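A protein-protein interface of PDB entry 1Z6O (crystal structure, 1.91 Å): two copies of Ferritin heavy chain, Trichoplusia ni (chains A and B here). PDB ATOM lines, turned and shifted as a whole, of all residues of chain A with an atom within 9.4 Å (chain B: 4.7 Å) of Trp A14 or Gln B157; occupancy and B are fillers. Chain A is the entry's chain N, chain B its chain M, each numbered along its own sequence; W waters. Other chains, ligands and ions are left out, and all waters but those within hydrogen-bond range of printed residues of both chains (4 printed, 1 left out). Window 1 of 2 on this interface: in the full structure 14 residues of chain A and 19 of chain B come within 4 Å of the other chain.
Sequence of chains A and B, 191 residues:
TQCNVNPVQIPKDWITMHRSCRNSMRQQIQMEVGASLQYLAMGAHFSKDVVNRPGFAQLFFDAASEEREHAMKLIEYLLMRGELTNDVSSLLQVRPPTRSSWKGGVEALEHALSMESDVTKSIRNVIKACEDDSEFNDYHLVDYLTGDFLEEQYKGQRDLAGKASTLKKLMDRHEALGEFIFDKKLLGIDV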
ATOM      1  N   GLN A   9      16.637  31.820  -0.112  1.00  0.00           N
ATOM      2  CA  GLN A   9      15.462  31.038   0.196  1.00  0.00           C
ATOM      3  C   GLN A   9      15.536  29.731  -0.562  1.00  0.00           C
ATOM      4  O   GLN A   9      15.934  29.708  -1.726  1.00  0.00           O
ATOM      5  CB  GLN A   9      14.205  31.796  -0.231  1.00  0.00           C
ATOM      6  CG  GLN A   9      14.035  33.164   0.421  1.00  0.00           C
ATOM      7  CD  GLN A   9      13.962  33.092   1.939  1.00  0.00           C
ATOM      8  OE1 GLN A   9      13.218  32.284   2.503  1.00  0.00           O
ATOM      9  NE2 GLN A   9      14.730  33.949   2.610  1.00  0.00           N
ATOM     10  N   ILE A  10      15.177  28.638   0.103  1.00  0.00           N
ATOM     11  CA  ILE A  10      15.160  27.349  -0.569  1.00  0.00           C
ATOM     12  C   ILE A  10      13.729  26.834  -0.392  1.00  0.00           C
ATOM     13  O   ILE A  10      12.944  27.424   0.350  1.00  0.00           O
ATOM     14  CB  ILE A  10      16.176  26.345   0.056  1.00  0.00           C
ATOM     15  CG1 ILE A  10      15.809  26.065   1.509  1.00  0.00           C
ATOM     16  CG2 ILE A  10      17.617  26.899  -0.050  1.00  0.00           C
ATOM     17  CD1 ILE A  10      16.469  24.792   2.057  1.00  0.00           C
ATOM     18  N   PRO A  11      13.370  25.734  -1.063  1.00  0.00           N
ATOM     19  CA  PRO A  11      12.021  25.156  -0.959  1.00  0.00           C
ATOM     20  C   PRO A  11      11.651  24.912   0.508  1.00  0.00           C
ATOM     21  O   PRO A  11      12.503  24.522   1.306  1.00  0.00           O
ATOM     22  CB  PRO A  11      12.145  23.848  -1.738  1.00  0.00           C
ATOM     23  CG  PRO A  11      13.194  24.181  -2.786  1.00  0.00           C
ATOM     24  CD  PRO A  11      14.218  24.948  -1.981  1.00  0.00           C
ATOM     25  N   LYS A  12      10.384  25.133   0.851  1.00  0.00           N
ATOM     26  CA  LYS A  12       9.910  24.962   2.220  1.00  0.00           C
ATOM     27  C   LYS A  12       8.761  23.979   2.388  1.00  0.00           C
ATOM     28  O   LYS A  12       8.263  23.812   3.498  1.00  0.00           O
ATOM     29  CB  LYS A  12       9.476  26.310   2.792  1.00  0.00           C
ATOM     30  CG  LYS A  12      10.613  27.308   2.933  1.00  0.00           C
ATOM     31  CD  LYS A  12      10.137  28.617   3.529  1.00  0.00           C
ATOM     32  CE  LYS A  12      11.274  29.630   3.562  1.00  0.00           C
ATOM     33  NZ  LYS A  12      10.879  30.905   4.228  1.00  0.00           N
ATOM     34  N   ASP A  13       8.334  23.326   1.314  1.00  0.00           N
ATOM     35  CA  ASP A  13       7.218  22.384   1.439  1.00  0.00           C
ATOM     36  C   ASP A  13       7.496  21.258   2.436  1.00  0.00           C
ATOM     37  O   ASP A  13       6.562  20.704   3.016  1.00  0.00           O
ATOM     38  CB  ASP A  13       6.863  21.756   0.089  1.00  0.00           C
ATOM     39  CG  ASP A  13       6.112  22.717  -0.827  1.00  0.00           C
ATOM     40  OD1 ASP A  13       5.603  23.750  -0.337  1.00  0.00           O
ATOM     41  OD2 ASP A  13       6.021  22.426  -2.039  1.00  0.00           O
ATOM     42  N   TRP A  14       8.769  20.916   2.623  1.00  0.00           N
ATOM     43  CA  TRP A  14       9.150  19.850   3.555  1.00  0.00           C
ATOM     44  C   TRP A  14       8.930  20.205   5.033  1.00  0.00           C
ATOM     45  O   TRP A  14       8.951  19.315   5.892  1.00  0.00           O
ATOM     46  CB  TRP A  14      10.633  19.479   3.357  1.00  0.00           C
ATOM     47  CG  TRP A  14      11.584  20.629   3.646  1.00  0.00           C
ATOM     48  CD1 TRP A  14      11.843  21.710   2.839  1.00  0.00           C
ATOM     49  CD2 TRP A  14      12.376  20.810   4.827  1.00  0.00           C
ATOM     50  NE1 TRP A  14      12.749  22.551   3.453  1.00  0.00           N
ATOM     51  CE2 TRP A  14      13.092  22.023   4.671  1.00  0.00           C
ATOM     52  CE3 TRP A  14      12.550  20.064   6.009  1.00  0.00           C
ATOM     53  CZ2 TRP A  14      13.971  22.513   5.654  1.00  0.00           C
ATOM     54  CZ3 TRP A  14      13.424  20.550   6.987  1.00  0.00           C
ATOM     55  CH2 TRP A  14      14.125  21.766   6.800  1.00  0.00           C
ATOM     56  N   ILE A  15       8.735  21.490   5.326  1.00  0.00           N
ATOM     57  CA  ILE A  15       8.547  21.976   6.709  1.00  0.00           C
ATOM     58  C   ILE A  15       7.064  21.848   6.999  1.00  0.00           C
ATOM     59  O   ILE A  15       6.275  22.666   6.555  1.00  0.00           O
ATOM     60  CB  ILE A  15       9.012  23.450   6.816  1.00  0.00           C
ATOM     61  CG1 ILE A  15      10.471  23.544   6.339  1.00  0.00           C
ATOM     62  CG2 ILE A  15       8.867  23.960   8.255  1.00  0.00           C
ATOM     63  CD1 ILE A  15      11.059  24.960   6.362  1.00  0.00           C
ATOM     64  N   THR A  16       6.685  20.843   7.780  1.00  0.00           N
ATOM     65  CA  THR A  16       5.266  20.556   7.973  1.00  0.00           C
ATOM     66  C   THR A  16       4.631  20.571   9.357  1.00  0.00           C
ATOM     67  O   THR A  16       3.438  20.324   9.469  1.00  0.00           O
ATOM     68  CB  THR A  16       4.969  19.176   7.382  1.00  0.00           C
ATOM     69  OG1 THR A  16       5.810  18.215   8.040  1.00  0.00           O
ATOM     70  CG2 THR A  16       5.284  19.136   5.879  1.00  0.00           C
ATOM     71  N   MET A  17       5.389  20.822  10.416  1.00  0.00           N
ATOM     72  CA  MET A  17       4.761  20.802  11.733  1.00  0.00           C
ATOM     73  C   MET A  17       3.666  21.858  11.840  1.00  0.00           C
ATOM     74  O   MET A  17       3.788  22.949  11.281  1.00  0.00           O
ATOM     75  CB  MET A  17       5.796  21.048  12.835  1.00  0.00           C
ATOM     76  CG  MET A  17       6.715  19.848  13.086  1.00  0.00           C
ATOM     77  SD  MET A  17       7.751  20.114  14.551  1.00  0.00           S
ATOM     78  CE  MET A  17       6.497  20.154  15.846  1.00  0.00           C
ATOM     79  N   TYR A  77      14.891  18.013  17.677  1.00  0.00           N
ATOM     80  CA  TYR A  77      13.808  17.485  16.846  1.00  0.00           C
ATOM     81  C   TYR A  77      13.173  18.648  16.060  1.00  0.00           C
ATOM     82  O   TYR A  77      12.953  18.551  14.853  1.00  0.00           O
ATOM     83  CB  TYR A  77      12.734  16.796  17.713  1.00  0.00           C
ATOM     84  CG  TYR A  77      11.699  16.101  16.857  1.00  0.00           C
ATOM     85  CD1 TYR A  77      11.854  14.760  16.503  1.00  0.00           C
ATOM     86  CD2 TYR A  77      10.644  16.821  16.284  1.00  0.00           C
ATOM     87  CE1 TYR A  77      10.989  14.149  15.585  1.00  0.00           C
ATOM     88  CE2 TYR A  77       9.774  16.223  15.362  1.00  0.00           C
ATOM     89  CZ  TYR A  77       9.961  14.890  15.015  1.00  0.00           C
ATOM     90  OH  TYR A  77       9.163  14.309  14.052  1.00  0.00           O
ATOM     91  N   LEU A  78      12.867  19.746  16.742  1.00  0.00           N
ATOM     92  CA  LEU A  78      12.275  20.897  16.053  1.00  0.00           C
ATOM     93  C   LEU A  78      13.199  21.400  14.933  1.00  0.00           C
ATOM     94  O   LEU A  78      12.740  21.729  13.839  1.00  0.00           O
ATOM     95  CB  LEU A  78      12.001  22.041  17.049  1.00  0.00           C
ATOM     96  CG  LEU A  78      10.935  21.759  18.128  1.00  0.00           C
ATOM     97  CD1 LEU A  78      10.754  22.999  19.005  1.00  0.00           C
ATOM     98  CD2 LEU A  78       9.601  21.385  17.468  1.00  0.00           C
ATOM     99  N   LEU A  79      14.500  21.461  15.205  1.00  0.00           N
ATOM    100  CA  LEU A  79      15.456  21.936  14.198  1.00  0.00           C
ATOM    101  C   LEU A  79      15.464  21.013  12.982  1.00  0.00           C
ATOM    102  O   LEU A  79      15.538  21.475  11.839  1.00  0.00           O
ATOM    103  CB  LEU A  79      16.874  22.012  14.794  1.00  0.00           C
ATOM    104  CG  LEU A  79      17.103  23.104  15.859  1.00  0.00           C
ATOM    105  CD1 LEU A  79      18.412  22.815  16.617  1.00  0.00           C
ATOM    106  CD2 LEU A  79      17.159  24.490  15.178  1.00  0.00           C
ATOM    107  N   MET A  80      15.401  19.705  13.225  1.00  0.00           N
ATOM    108  CA  MET A  80      15.398  18.736  12.129  1.00  0.00           C
ATOM    109  C   MET A  80      14.172  18.929  11.228  1.00  0.00           C
ATOM    110  O   MET A  80      14.252  18.727  10.012  1.00  0.00           O
ATOM    111  CB  MET A  80      15.397  17.296  12.677  1.00  0.00           C
ATOM    112  CG  MET A  80      15.142  16.236  11.591  1.00  0.00           C
ATOM    113  SD  MET A  80      15.015  14.542  12.229  1.00  0.00           S
ATOM    114  CE  MET A  80      13.340  14.645  13.018  1.00  0.00           C
ATOM    115  N   ARG A  81      13.043  19.309  11.825  1.00  0.00           N
ATOM    116  CA  ARG A  81      11.803  19.519  11.069  1.00  0.00           C
ATOM    117  C   ARG A  81      11.743  20.880  10.361  1.00  0.00           C
ATOM    118  O   ARG A  81      10.758  21.192   9.685  1.00  0.00           O
ATOM    119  CB  ARG A  81      10.578  19.336  11.991  1.00  0.00           C
ATOM    120  CG  ARG A  81      10.378  17.872  12.461  1.00  0.00           C
ATOM    121  CD  ARG A  81       9.984  16.947  11.288  1.00  0.00           C
ATOM    122  NE  ARG A  81       8.644  17.264  10.777  1.00  0.00           N
ATOM    123  CZ  ARG A  81       7.498  16.834  11.312  1.00  0.00           C
ATOM    124  NH1 ARG A  81       7.500  16.044  12.385  1.00  0.00           N
ATOM    125  NH2 ARG A  81       6.335  17.213  10.783  1.00  0.00           N
ATOM    126  N   GLY A  82      12.788  21.689  10.515  1.00  0.00           N
ATOM    127  CA  GLY A  82      12.814  22.976   9.829  1.00  0.00           C
ATOM    128  C   GLY A  82      12.335  24.152  10.657  1.00  0.00           C
ATOM    129  O   GLY A  82      12.153  25.250  10.128  1.00  0.00           O
ATOM    130  N   GLU A  83      12.140  23.937  11.954  1.00  0.00           N
ATOM    131  CA  GLU A  83      11.674  25.005  12.834  1.00  0.00           C
ATOM    132  C   GLU A  83      12.831  25.755  13.485  1.00  0.00           C
ATOM    133  O   GLU A  83      14.002  25.472  13.230  1.00  0.00           O
ATOM    134  CB  GLU A  83      10.775  24.422  13.932  1.00  0.00           C
ATOM    135  CG  GLU A  83       9.533  23.692  13.400  1.00  0.00           C
ATOM    136  CD  GLU A  83       8.558  24.640  12.683  1.00  0.00           C
ATOM    137  OE1 GLU A  83       8.590  25.857  12.964  1.00  0.00           O
ATOM    138  OE2 GLU A  83       7.750  24.169  11.856  1.00  0.00           O
ATOM    139  N   LEU A  84      12.473  26.718  14.329  1.00  0.00           N
ATOM    140  CA  LEU A  84      13.423  27.541  15.067  1.00  0.00           C
ATOM    141  C   LEU A  84      14.360  28.386  14.209  1.00  0.00           C
ATOM    142  O   LEU A  84      15.534  28.559  14.538  1.00  0.00           O
ATOM    143  CB  LEU A  84      14.218  26.676  16.066  1.00  0.00           C
ATOM    144  CG  LEU A  84      13.327  25.965  17.103  1.00  0.00           C
ATOM    145  CD1 LEU A  84      14.188  25.170  18.090  1.00  0.00           C
ATOM    146  CD2 LEU A  84      12.481  27.008  17.862  1.00  0.00           C
ATOM    147  N   THR A  85      13.840  28.897  13.096  1.00  0.00           N
ATOM    148  CA  THR A  85      14.608  29.814  12.261  1.00  0.00           C
ATOM    149  C   THR A  85      14.423  31.200  12.913  1.00  0.00           C
ATOM    150  O   THR A  85      15.079  32.168  12.544  1.00  0.00           O
ATOM    151  CB  THR A  85      14.099  29.837  10.820  1.00  0.00           C
ATOM    152  OG1 THR A  85      12.673  29.963  10.823  1.00  0.00           O
ATOM    153  CG2 THR A  85      14.502  28.537  10.110  1.00  0.00           C
ATOM    154  N   PHE A 136      -3.513  17.847  10.668  1.00  0.00           N
ATOM    155  CA  PHE A 136      -2.247  17.141  10.448  1.00  0.00           C
ATOM    156  C   PHE A 136      -1.897  16.249  11.635  1.00  0.00           C
ATOM    157  O   PHE A 136      -1.656  16.742  12.733  1.00  0.00           O
ATOM    158  CB  PHE A 136      -1.136  18.189  10.255  1.00  0.00           C
ATOM    159  CG  PHE A 136       0.189  17.624   9.793  1.00  0.00           C
ATOM    160  CD1 PHE A 136       0.437  17.412   8.437  1.00  0.00           C
ATOM    161  CD2 PHE A 136       1.197  17.335  10.716  1.00  0.00           C
ATOM    162  CE1 PHE A 136       1.681  16.920   7.997  1.00  0.00           C
ATOM    163  CE2 PHE A 136       2.445  16.843  10.294  1.00  0.00           C
ATOM    164  CZ  PHE A 136       2.688  16.634   8.930  1.00  0.00           C
ATOM    165  N   ASP A 138       0.770  14.285  13.239  1.00  0.00           N
ATOM    166  CA  ASP A 138       2.224  14.188  13.087  1.00  0.00           C
ATOM    167  C   ASP A 138       2.718  12.813  13.528  1.00  0.00           C
ATOM    168  O   ASP A 138       3.259  12.649  14.627  1.00  0.00           O
ATOM    169  CB  ASP A 138       2.908  15.283  13.901  1.00  0.00           C
ATOM    170  CG  ASP A 138       4.255  15.662  13.319  1.00  0.00           C
ATOM    171  OD1 ASP A 138       5.051  14.736  13.014  1.00  0.00           O
ATOM    172  OD2 ASP A 138       4.511  16.872  13.154  1.00  0.00           O
ATOM    173  N   HIS A 140       5.298  10.867  12.887  1.00  0.00           N
ATOM    174  CA  HIS A 140       6.672  10.683  13.312  1.00  0.00           C
ATOM    175  C   HIS A 140       6.999  11.256  14.683  1.00  0.00           C
ATOM    176  O   HIS A 140       7.654  10.591  15.489  1.00  0.00           O
ATOM    177  CB  HIS A 140       7.634  11.242  12.265  1.00  0.00           C
ATOM    178  CG  HIS A 140       9.070  10.951  12.575  1.00  0.00           C
ATOM    179  ND1 HIS A 140       9.903  11.875  13.171  1.00  0.00           N
ATOM    180  CD2 HIS A 140       9.804   9.820  12.428  1.00  0.00           C
ATOM    181  CE1 HIS A 140      11.091  11.327  13.378  1.00  0.00           C
ATOM    182  NE2 HIS A 140      11.057  10.080  12.937  1.00  0.00           N
ATOM    183  N   LEU B 113      15.341  17.673  -2.581  1.00  0.00           N
ATOM    184  CA  LEU B 113      14.555  18.003  -1.387  1.00  0.00           C
ATOM    185  C   LEU B 113      13.055  17.913  -1.701  1.00  0.00           C
ATOM    186  O   LEU B 113      12.273  17.381  -0.917  1.00  0.00           O
ATOM    187  CB  LEU B 113      14.906  19.417  -0.894  1.00  0.00           C
ATOM    188  CG  LEU B 113      14.124  19.984   0.304  1.00  0.00           C
ATOM    189  CD1 LEU B 113      14.225  19.034   1.511  1.00  0.00           C
ATOM    190  CD2 LEU B 113      14.697  21.373   0.660  1.00  0.00           C
ATOM    191  N   GLU B 116      12.026  14.267  -2.050  1.00  0.00           N
ATOM    192  CA  GLU B 116      11.919  13.634  -0.732  1.00  0.00           C
ATOM    193  C   GLU B 116      10.651  14.098  -0.020  1.00  0.00           C
ATOM    194  O   GLU B 116       9.962  13.310   0.621  1.00  0.00           O
ATOM    195  CB  GLU B 116      13.150  13.950   0.131  1.00  0.00           C
ATOM    196  CG  GLU B 116      14.442  13.288  -0.373  1.00  0.00           C
ATOM    197  CD  GLU B 116      14.306  11.770  -0.560  1.00  0.00           C
ATOM    198  OE1 GLU B 116      13.574  11.125   0.222  1.00  0.00           O
ATOM    199  OE2 GLU B 116      14.943  11.213  -1.486  1.00  0.00           O
ATOM    200  N   SER B 117      10.354  15.385  -0.141  1.00  0.00           N
ATOM    201  CA  SER B 117       9.160  15.970   0.461  1.00  0.00           C
ATOM    202  C   SER B 117       7.904  15.262  -0.109  1.00  0.00           C
ATOM    203  O   SER B 117       6.947  14.966   0.624  1.00  0.00           O
ATOM    204  CB  SER B 117       9.149  17.493   0.154  1.00  0.00           C
ATOM    205  OG  SER B 117       7.999  18.102   0.689  1.00  0.00           O
ATOM    206  N   THR B 120       7.683  11.785   1.414  1.00  0.00           N
ATOM    207  CA  THR B 120       7.225  11.842   2.804  1.00  0.00           C
ATOM    208  C   THR B 120       5.702  11.969   2.851  1.00  0.00           C
ATOM    209  O   THR B 120       5.020  11.290   3.621  1.00  0.00           O
ATOM    210  CB  THR B 120       7.860  13.038   3.531  1.00  0.00           C
ATOM    211  OG1 THR B 120       9.283  12.887   3.498  1.00  0.00           O
ATOM    212  CG2 THR B 120       7.386  13.116   4.998  1.00  0.00           C
ATOM    213  N   GLN B 153      13.026   9.647   6.191  1.00  0.00           N
ATOM    214  CA  GLN B 153      12.587  10.812   5.420  1.00  0.00           C
ATOM    215  C   GLN B 153      12.897  12.136   6.097  1.00  0.00           C
ATOM    216  O   GLN B 153      13.442  13.040   5.464  1.00  0.00           O
ATOM    217  CB  GLN B 153      11.071  10.769   5.153  1.00  0.00           C
ATOM    218  CG  GLN B 153      10.632   9.735   4.107  1.00  0.00           C
ATOM    219  CD  GLN B 153      11.458   9.827   2.838  1.00  0.00           C
ATOM    220  OE1 GLN B 153      12.264   8.944   2.553  1.00  0.00           O
ATOM    221  NE2 GLN B 153      11.282  10.914   2.082  1.00  0.00           N
ATOM    222  N   TYR B 154      12.541  12.272   7.375  1.00  0.00           N
ATOM    223  CA  TYR B 154      12.775  13.551   8.039  1.00  0.00           C
ATOM    224  C   TYR B 154      14.246  13.880   8.192  1.00  0.00           C
ATOM    225  O   TYR B 154      14.642  15.031   8.007  1.00  0.00           O
ATOM    226  CB  TYR B 154      12.041  13.616   9.388  1.00  0.00           C
ATOM    227  CG  TYR B 154      10.535  13.735   9.208  1.00  0.00           C
ATOM    228  CD1 TYR B 154       9.683  12.694   9.577  1.00  0.00           C
ATOM    229  CD2 TYR B 154       9.967  14.880   8.628  1.00  0.00           C
ATOM    230  CE1 TYR B 154       8.294  12.782   9.369  1.00  0.00           C
ATOM    231  CE2 TYR B 154       8.582  14.981   8.423  1.00  0.00           C
ATOM    232  CZ  TYR B 154       7.754  13.923   8.798  1.00  0.00           C
ATOM    233  OH  TYR B 154       6.391  14.011   8.613  1.00  0.00           O
ATOM    234  N   LYS B 155      15.067  12.883   8.511  1.00  0.00           N
ATOM    235  CA  LYS B 155      16.505  13.128   8.634  1.00  0.00           C
ATOM    236  C   LYS B 155      17.067  13.521   7.266  1.00  0.00           C
ATOM    237  O   LYS B 155      17.888  14.437   7.158  1.00  0.00           O
ATOM    238  CB  LYS B 155      17.234  11.866   9.119  1.00  0.00           C
ATOM    239  CG  LYS B 155      16.980  11.528  10.577  1.00  0.00           C
ATOM    240  CD  LYS B 155      17.814  10.320  11.011  1.00  0.00           C
ATOM    241  CE  LYS B 155      17.554   9.099  10.123  1.00  0.00           C
ATOM    242  NZ  LYS B 155      18.295   7.885  10.571  1.00  0.00           N
ATOM    243  N   GLY B 156      16.623  12.818   6.225  1.00  0.00           N
ATOM    244  CA  GLY B 156      17.099  13.096   4.874  1.00  0.00           C
ATOM    245  C   GLY B 156      16.735  14.492   4.388  1.00  0.00           C
ATOM    246  O   GLY B 156      17.545  15.165   3.748  1.00  0.00           O
ATOM    247  N   GLN B 157      15.509  14.925   4.667  1.00  0.00           N
ATOM    248  CA  GLN B 157      15.069  16.262   4.264  1.00  0.00           C
ATOM    249  C   GLN B 157      15.910  17.328   4.950  1.00  0.00           C
ATOM    250  O   GLN B 157      16.350  18.282   4.317  1.00  0.00           O
ATOM    251  CB  GLN B 157      13.587  16.488   4.635  1.00  0.00           C
ATOM    252  CG  GLN B 157      12.636  15.675   3.783  1.00  0.00           C
ATOM    253  CD  GLN B 157      11.190  15.740   4.255  1.00  0.00           C
ATOM    254  OE1 GLN B 157      10.873  16.210   5.365  1.00  0.00           O
ATOM    255  NE2 GLN B 157      10.311  15.251   3.424  1.00  0.00           N
ATOM    256  N   ARG B 158      16.130  17.173   6.254  1.00  0.00           N
ATOM    257  CA  ARG B 158      16.914  18.166   6.979  1.00  0.00           C
ATOM    258  C   ARG B 158      18.330  18.225   6.417  1.00  0.00           C
ATOM    259  O   ARG B 158      18.914  19.302   6.294  1.00  0.00           O
ATOM    260  CB  ARG B 158      16.962  17.834   8.478  1.00  0.00           C
ATOM    261  CG  ARG B 158      17.905  18.758   9.294  1.00  0.00           C
ATOM    262  CD  ARG B 158      17.495  20.252   9.249  1.00  0.00           C
ATOM    263  NE  ARG B 158      18.468  21.068   9.987  1.00  0.00           N
ATOM    264  CZ  ARG B 158      19.639  21.471   9.504  1.00  0.00           C
ATOM    265  NH1 ARG B 158      19.994  21.158   8.257  1.00  0.00           N
ATOM    266  NH2 ARG B 158      20.487  22.147  10.284  1.00  0.00           N
ATOM    267  N   ASP B 159      18.885  17.067   6.080  1.00  0.00           N
ATOM    268  CA  ASP B 159      20.237  17.033   5.529  1.00  0.00           C
ATOM    269  C   ASP B 159      20.301  17.778   4.190  1.00  0.00           C
ATOM    270  O   ASP B 159      21.169  18.630   3.990  1.00  0.00           O
ATOM    271  CB  ASP B 159      20.699  15.590   5.347  1.00  0.00           C
ATOM    272  CG  ASP B 159      22.140  15.508   4.869  1.00  0.00           C
ATOM    273  OD1 ASP B 159      22.359  15.094   3.720  1.00  0.00           O
ATOM    274  OD2 ASP B 159      23.051  15.878   5.639  1.00  0.00           O
ATOM    275  N   LEU B 160      19.379  17.467   3.279  1.00  0.00           N
ATOM    276  CA  LEU B 160      19.342  18.137   1.972  1.00  0.00           C
ATOM    277  C   LEU B 160      19.054  19.630   2.094  1.00  0.00           C
ATOM    278  O   LEU B 160      19.639  20.438   1.370  1.00  0.00           O
ATOM    279  CB  LEU B 160      18.272  17.508   1.071  1.00  0.00           C
ATOM    280  CG  LEU B 160      18.589  16.096   0.558  1.00  0.00           C
ATOM    281  CD1 LEU B 160      17.329  15.486  -0.079  1.00  0.00           C
ATOM    282  CD2 LEU B 160      19.738  16.171  -0.466  1.00  0.00           C
ATOM    283  N   ALA B 161      18.137  20.000   2.989  1.00  0.00           N
ATOM    284  CA  ALA B 161      17.799  21.416   3.171  1.00  0.00           C
ATOM    285  C   ALA B 161      19.028  22.191   3.656  1.00  0.00           C
ATOM    286  O   ALA B 161      19.283  23.307   3.201  1.00  0.00           O
ATOM    287  CB  ALA B 161      16.648  21.567   4.184  1.00  0.00           C
HETATM  288  O   HOH W   1       5.135  18.610   2.131  1.00  0.00           O
HETATM  289  O   HOH W   2       5.716  15.860   6.903  1.00  0.00           O
HETATM  290  O   HOH W   3       7.902  16.784   5.320  1.00  0.00           O
HETATM  291  O   HOH W   4       4.826  13.174  10.791  1.00  0.00           O
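OG of Ser B117 sits close to N of Trp A14 (3.5 Å).
The guanidinium group of Arg B158 sits close to the backbone carbonyl oxygen of Leu A79, at 3.5 Å.
O of Glu B116 is in hydrogen-bond range of NE2 of Gln B157, at 3.4 Å.
NE2 of Gln B157 is in hydrogen-bond range of OG1 of Thr B120 (2.6 Å).
NE1 of Trp A14 sits at hydrogen-bond distance from O of Pro A11 (2.9 Å).
The side-chain hydroxyl of Thr A16 sits at hydrogen-bond distance from the guanidinium group of Arg A81, at 3.0 Å.
NH1 of Arg A81 sits at hydrogen-bond distance from OH of Tyr A77.
The guanidinium group (NH1) of Arg A81 is in salt-bridge range of the side-chain carboxylate (OD1) of Asp A138, at 2.8 Å.
Among the printed residues, merely in contact across the chains: Ile A10 with Ala B161 (3.4 Å), Pro A11 with Leu B113 (3.9 Å), Asp A13 with Ser B117 (3.6 Å), Trp A14 with Leu B113 (3.6 Å), Trp A14 with Gln B157 (3.7 Å), Trp A14 with Ala B161 (3.2 Å), Met A80 with Tyr B154 (3.8 Å), Met A80 with Lys B155 (3.96 Å), Met A80 with Arg B158 (3.2 Å), Arg A81 with Tyr B154 (3.3 Å) and His A140 with Tyr B154 (3.3 Å).
Of chain B, only Leu B113 (3.6 Å), Ser B117 (3.5 Å), Gln B157 (3.7 Å) and Ala B161 (3.2 Å) come within 4 Å of Trp A14.
Of chain A, only Trp A14 comes within 4 Å of Gln B157.
Of the printed residues of chain A, Ser B117 touches Asp A13 and Trp A14.
No residue of chain A comes within 4 Å of Gly B156.
Printed residues of chain A within 4 Å of Ala B161: Ile A10 and Trp A14.
Of the printed residues of chain A, Leu B113 touches Pro A11 and Trp A14.
Of the printed residues of chain A, Arg B158 touches Leu A79 (3.5 Å) and Met A80 (3.2 Å).
The nearest residue of chain A that does not touch Gln B157 is Met A80 (5.5 Å).
The nearest printed residue of chain B that does not touch Ile A10 is Leu B113 (4.1 Å).
Printed residues of chain B that touch a printed residue of chain A: Leu B113, Ser B117, Tyr B154, Lys B155, Gln B157, Arg B158 and Ala B161.
Hydrophobic or aromatic side chains of chain B that line the printed part of chain A: Leu B113, Tyr B154 and Ala B161.
Along chain B the printed residues that touch a printed residue of chain A span positions 113 to 161.
Among the printed residues, 13 pairs touch across the chains.
No position is printed for both chains.
Water W2 bridges the side-chain hydroxyl (OH) of Tyr B154 (2.6 Å) and the side-chain hydroxyl (OG1) of Thr A16 (2.6 Å).
Water W1 bridges the backbone carbonyl oxygen (O) of Asp A13 and the side-chain hydroxyl (OG) of Ser B117.
Water W4 lies within hydrogen-bond range of OD1 of Asp A138, OH of Tyr B154 and N of His A140.
Water W3 bridges the backbone carbonyl oxygen of Trp A14 and the side-chain amide oxygen of Gln B157.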
